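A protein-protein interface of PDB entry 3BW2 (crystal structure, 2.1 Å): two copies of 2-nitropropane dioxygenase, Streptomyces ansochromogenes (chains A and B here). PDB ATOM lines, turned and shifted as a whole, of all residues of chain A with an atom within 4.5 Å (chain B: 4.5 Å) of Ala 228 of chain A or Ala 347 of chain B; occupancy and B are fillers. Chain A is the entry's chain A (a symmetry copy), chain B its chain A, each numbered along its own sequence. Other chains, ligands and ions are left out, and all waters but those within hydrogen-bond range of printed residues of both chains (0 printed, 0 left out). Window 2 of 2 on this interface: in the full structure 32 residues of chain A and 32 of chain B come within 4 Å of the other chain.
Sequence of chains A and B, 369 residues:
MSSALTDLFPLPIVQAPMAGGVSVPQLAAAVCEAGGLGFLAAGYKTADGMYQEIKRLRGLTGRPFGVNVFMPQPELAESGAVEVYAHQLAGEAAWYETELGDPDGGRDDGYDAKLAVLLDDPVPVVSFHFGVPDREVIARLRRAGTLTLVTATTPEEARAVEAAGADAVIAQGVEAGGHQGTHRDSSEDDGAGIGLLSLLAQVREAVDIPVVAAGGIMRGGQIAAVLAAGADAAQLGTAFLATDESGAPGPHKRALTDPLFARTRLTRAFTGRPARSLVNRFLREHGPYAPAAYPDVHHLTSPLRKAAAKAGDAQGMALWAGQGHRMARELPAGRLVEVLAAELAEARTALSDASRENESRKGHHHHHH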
ATOM      1  N   ALA A 224       4.979 -22.316  33.039  1.00  0.00           N
ATOM      2  CA  ALA A 224       5.021 -23.562  32.277  1.00  0.00           C
ATOM      3  C   ALA A 224       6.371 -23.643  31.573  1.00  0.00           C
ATOM      4  O   ALA A 224       6.961 -24.718  31.451  1.00  0.00           O
ATOM      5  CB  ALA A 224       3.895 -23.591  31.244  1.00  0.00           C
ATOM      6  N   ALA A 225       6.854 -22.494  31.111  1.00  0.00           N
ATOM      7  CA  ALA A 225       8.130 -22.428  30.422  1.00  0.00           C
ATOM      8  C   ALA A 225       9.271 -22.928  31.302  1.00  0.00           C
ATOM      9  O   ALA A 225      10.046 -23.789  30.883  1.00  0.00           O
ATOM     10  CB  ALA A 225       8.410 -20.990  29.965  1.00  0.00           C
ATOM     11  N   VAL A 226       9.384 -22.397  32.517  1.00  0.00           N
ATOM     12  CA  VAL A 226      10.469 -22.824  33.401  1.00  0.00           C
ATOM     13  C   VAL A 226      10.342 -24.282  33.818  1.00  0.00           C
ATOM     14  O   VAL A 226      11.351 -24.962  34.021  1.00  0.00           O
ATOM     15  CB  VAL A 226      10.577 -21.934  34.667  1.00  0.00           C
ATOM     16  CG1 VAL A 226      10.883 -20.498  34.260  1.00  0.00           C
ATOM     17  CG2 VAL A 226       9.291 -22.007  35.486  1.00  0.00           C
ATOM     18  N   LEU A 227       9.111 -24.769  33.947  1.00  0.00           N
ATOM     19  CA  LEU A 227       8.903 -26.163  34.321  1.00  0.00           C
ATOM     20  C   LEU A 227       9.425 -27.045  33.190  1.00  0.00           C
ATOM     21  O   LEU A 227      10.095 -28.053  33.427  1.00  0.00           O
ATOM     22  CB  LEU A 227       7.414 -26.440  34.559  1.00  0.00           C
ATOM     23  CG  LEU A 227       6.770 -25.730  35.755  1.00  0.00           C
ATOM     24  CD1 LEU A 227       5.302 -26.129  35.867  1.00  0.00           C
ATOM     25  CD2 LEU A 227       7.517 -26.091  37.029  1.00  0.00           C
ATOM     26  N   ALA A 228       9.120 -26.649  31.959  1.00  0.00           N
ATOM     27  CA  ALA A 228       9.559 -27.385  30.782  1.00  0.00           C
ATOM     28  C   ALA A 228      11.079 -27.413  30.723  1.00  0.00           C
ATOM     29  O   ALA A 228      11.670 -28.375  30.236  1.00  0.00           O
ATOM     30  CB  ALA A 228       9.006 -26.734  29.517  1.00  0.00           C
ATOM     31  N   ALA A 229      11.706 -26.353  31.226  1.00  0.00           N
ATOM     32  CA  ALA A 229      13.159 -26.252  31.215  1.00  0.00           C
ATOM     33  C   ALA A 229      13.852 -26.913  32.407  1.00  0.00           C
ATOM     34  O   ALA A 229      15.068 -26.801  32.554  1.00  0.00           O
ATOM     35  CB  ALA A 229      13.572 -24.792  31.113  1.00  0.00           C
ATOM     36  N   GLY A 230      13.097 -27.588  33.268  1.00  0.00           N
ATOM     37  CA  GLY A 230      13.725 -28.258  34.397  1.00  0.00           C
ATOM     38  C   GLY A 230      13.446 -27.746  35.800  1.00  0.00           C
ATOM     39  O   GLY A 230      13.882 -28.365  36.777  1.00  0.00           O
ATOM     40  N   GLY B 221      14.679 -28.947  25.864  1.00  0.00           N
ATOM     41  CA  GLY B 221      13.806 -28.507  26.945  1.00  0.00           C
ATOM     42  C   GLY B 221      13.578 -27.005  26.911  1.00  0.00           C
ATOM     43  O   GLY B 221      12.524 -26.509  27.317  1.00  0.00           O
ATOM     44  N   ALA B 224      11.007 -26.336  24.314  1.00  0.00           N
ATOM     45  CA  ALA B 224       9.675 -26.570  24.867  1.00  0.00           C
ATOM     46  C   ALA B 224       9.301 -25.370  25.729  1.00  0.00           C
ATOM     47  O   ALA B 224       8.145 -24.945  25.759  1.00  0.00           O
ATOM     48  CB  ALA B 224       9.667 -27.841  25.716  1.00  0.00           C
ATOM     49  N   ALA B 225      10.292 -24.829  26.431  1.00  0.00           N
ATOM     50  CA  ALA B 225      10.075 -23.680  27.292  1.00  0.00           C
ATOM     51  C   ALA B 225       9.540 -22.483  26.511  1.00  0.00           C
ATOM     52  O   ALA B 225       8.525 -21.897  26.891  1.00  0.00           O
ATOM     53  CB  ALA B 225      11.379 -23.302  28.006  1.00  0.00           C
ATOM     54  N   GLU B 343      14.828 -34.251  22.896  1.00  0.00           N
ATOM     55  CA  GLU B 343      14.780 -33.522  24.158  1.00  0.00           C
ATOM     56  C   GLU B 343      13.473 -32.747  24.241  1.00  0.00           C
ATOM     57  O   GLU B 343      12.856 -32.659  25.306  1.00  0.00           O
ATOM     58  CB  GLU B 343      15.988 -32.589  24.272  1.00  0.00           C
ATOM     59  CG  GLU B 343      17.302 -33.344  24.490  1.00  0.00           C
ATOM     60  CD  GLU B 343      18.527 -32.450  24.406  1.00  0.00           C
ATOM     61  OE1 GLU B 343      19.618 -32.907  24.804  1.00  0.00           O
ATOM     62  OE2 GLU B 343      18.408 -31.300  23.932  1.00  0.00           O
ATOM     63  N   LEU B 344      13.051 -32.200  23.104  1.00  0.00           N
ATOM     64  CA  LEU B 344      11.799 -31.459  23.021  1.00  0.00           C
ATOM     65  C   LEU B 344      10.635 -32.376  23.390  1.00  0.00           C
ATOM     66  O   LEU B 344       9.803 -32.034  24.231  1.00  0.00           O
ATOM     67  CB  LEU B 344      11.596 -30.929  21.601  1.00  0.00           C
ATOM     68  CG  LEU B 344      10.229 -30.326  21.267  1.00  0.00           C
ATOM     69  CD1 LEU B 344       9.956 -29.142  22.179  1.00  0.00           C
ATOM     70  CD2 LEU B 344      10.203 -29.889  19.810  1.00  0.00           C
ATOM     71  N   ALA B 345      10.580 -33.543  22.756  1.00  0.00           N
ATOM     72  CA  ALA B 345       9.512 -34.500  23.023  1.00  0.00           C
ATOM     73  C   ALA B 345       9.528 -34.919  24.490  1.00  0.00           C
ATOM     74  O   ALA B 345       8.485 -34.993  25.134  1.00  0.00           O
ATOM     75  CB  ALA B 345       9.671 -35.725  22.125  1.00  0.00           C
ATOM     76  N   GLU B 346      10.718 -35.185  25.014  1.00  0.00           N
ATOM     77  CA  GLU B 346      10.862 -35.592  26.405  1.00  0.00           C
ATOM     78  C   GLU B 346      10.316 -34.521  27.347  1.00  0.00           C
ATOM     79  O   GLU B 346       9.644 -34.834  28.331  1.00  0.00           O
ATOM     80  CB  GLU B 346      12.332 -35.863  26.722  1.00  0.00           C
ATOM     81  CG  GLU B 346      12.624 -36.029  28.201  1.00  0.00           C
ATOM     82  CD  GLU B 346      14.102 -36.206  28.486  1.00  0.00           C
ATOM     83  OE1 GLU B 346      14.911 -35.401  27.966  1.00  0.00           O
ATOM     84  OE2 GLU B 346      14.456 -37.143  29.235  1.00  0.00           O
ATOM     85  N   ALA B 347      10.606 -33.257  27.045  1.00  0.00           N
ATOM     86  CA  ALA B 347      10.128 -32.155  27.873  1.00  0.00           C
ATOM     87  C   ALA B 347       8.612 -32.010  27.755  1.00  0.00           C
ATOM     88  O   ALA B 347       7.936 -31.744  28.743  1.00  0.00           O
ATOM     89  CB  ALA B 347      10.818 -30.852  27.469  1.00  0.00           C
ATOM     90  N   ARG B 348       8.080 -32.186  26.548  1.00  0.00           N
ATOM     91  CA  ARG B 348       6.635 -32.085  26.334  1.00  0.00           C
ATOM     92  C   ARG B 348       5.916 -33.078  27.233  1.00  0.00           C
ATOM     93  O   ARG B 348       5.000 -32.721  27.972  1.00  0.00           O
ATOM     94  CB  ARG B 348       6.272 -32.407  24.886  1.00  0.00           C
ATOM     95  CG  ARG B 348       6.464 -31.291  23.889  1.00  0.00           C
ATOM     96  CD  ARG B 348       6.117 -31.803  22.495  1.00  0.00           C
ATOM     97  NE  ARG B 348       6.201 -30.762  21.476  1.00  0.00           N
ATOM     98  CZ  ARG B 348       5.376 -29.723  21.403  1.00  0.00           C
ATOM     99  NH1 ARG B 348       4.402 -29.584  22.290  1.00  0.00           N
ATOM    100  NH2 ARG B 348       5.526 -28.823  20.442  1.00  0.00           N
ATOM    101  N   THR B 349       6.336 -34.335  27.147  1.00  0.00           N
ATOM    102  CA  THR B 349       5.746 -35.400  27.942  1.00  0.00           C
ATOM    103  C   THR B 349       5.769 -35.061  29.430  1.00  0.00           C
ATOM    104  O   THR B 349       4.763 -35.221  30.122  1.00  0.00           O
ATOM    105  CB  THR B 349       6.492 -36.725  27.710  1.00  0.00           C
ATOM    106  OG1 THR B 349       6.401 -37.085  26.327  1.00  0.00           O
ATOM    107  CG2 THR B 349       5.887 -37.834  28.552  1.00  0.00           C
ATOM    108  N   ALA B 350       6.914 -34.589  29.915  1.00  0.00           N
ATOM    109  CA  ALA B 350       7.060 -34.232  31.323  1.00  0.00           C
ATOM    110  C   ALA B 350       6.018 -33.201  31.751  1.00  0.00           C
ATOM    111  O   ALA B 350       5.420 -33.325  32.818  1.00  0.00           O
ATOM    112  CB  ALA B 350       8.461 -33.698  31.580  1.00  0.00           C
ATOM    113  N   LEU B 351       5.803 -32.187  30.916  1.00  0.00           N
ATOM    114  CA  LEU B 351       4.824 -31.140  31.211  1.00  0.00           C
ATOM    115  C   LEU B 351       3.404 -31.698  31.243  1.00  0.00           C
ATOM    116  O   LEU B 351       2.440 -30.950  31.407  1.00  0.00           O
ATOM    117  CB  LEU B 351       4.889 -30.025  30.162  1.00  0.00           C
ATOM    118  CG  LEU B 351       5.357 -28.631  30.590  1.00  0.00           C
ATOM    119  CD1 LEU B 351       5.121 -27.661  29.442  1.00  0.00           C
ATOM    120  CD2 LEU B 351       4.600 -28.165  31.823  1.00  0.00           C
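Printed residues of chain A that touch a printed residue of chain B: Ala 225, Ala 228 and Ala 229.
Hydrophobic or aromatic side chains of chain A within 4 Å of the printed part of chain B: Ala 225 and Ala 228.
Of the 12 printed residues of chain B, 4 touch a printed residue of chain A.
Among the printed residues, no Asp or Glu carboxylate lies within 4 Å of a Lys or Arg side-chain nitrogen of the other chain.
Among the printed residues, pairs that only touch across the chains: Ala 225 of chain A with Ala 225 of chain B (3.2 Å), Ala 228 of chain A with Gly 221 of chain B (3.6 Å), Ala 228 of chain A with Ala 347 of chain B (3.8 Å), Ala 228 of chain A with Ala 225 of chain B (3.8 Å), Ala 229 of chain A with Gly 221 of chain B (3.96 Å) and Ala 228 of chain A with Leu 351 of chain B (3.99 Å).
Of the printed residues of chain B, Ala 228 of chain A touches Gly 221 (3.6 Å), Ala 225 (3.8 Å), Ala 347 (3.8 Å) and Leu 351 (3.99 Å).
Of the printed residues of chain A, Gly 221 of chain B touches Ala 228 (3.6 Å) and Ala 229 (3.96 Å).
Of the printed residues of chain A, Leu 351 of chain B touches Ala 228.
Of the printed residues of chain A, Ala 225 of chain B touches Ala 225 (3.2 Å) and Ala 228 (3.8 Å).
Printed residues of chain B within 4 Å of Ala 229 of chain A: Gly 221 (3.96 Å).
The nearest printed residue of chain A that does not touch Ala 347 of chain B is Ala 229 of chain A (5.9 Å).
Ala 225 of chain B touches its own counterpart, Ala 225 of chain A.
Of the 6 pairs that touch across the chains among the printed residues, 1 has its exchanged pair printed and touching as well.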
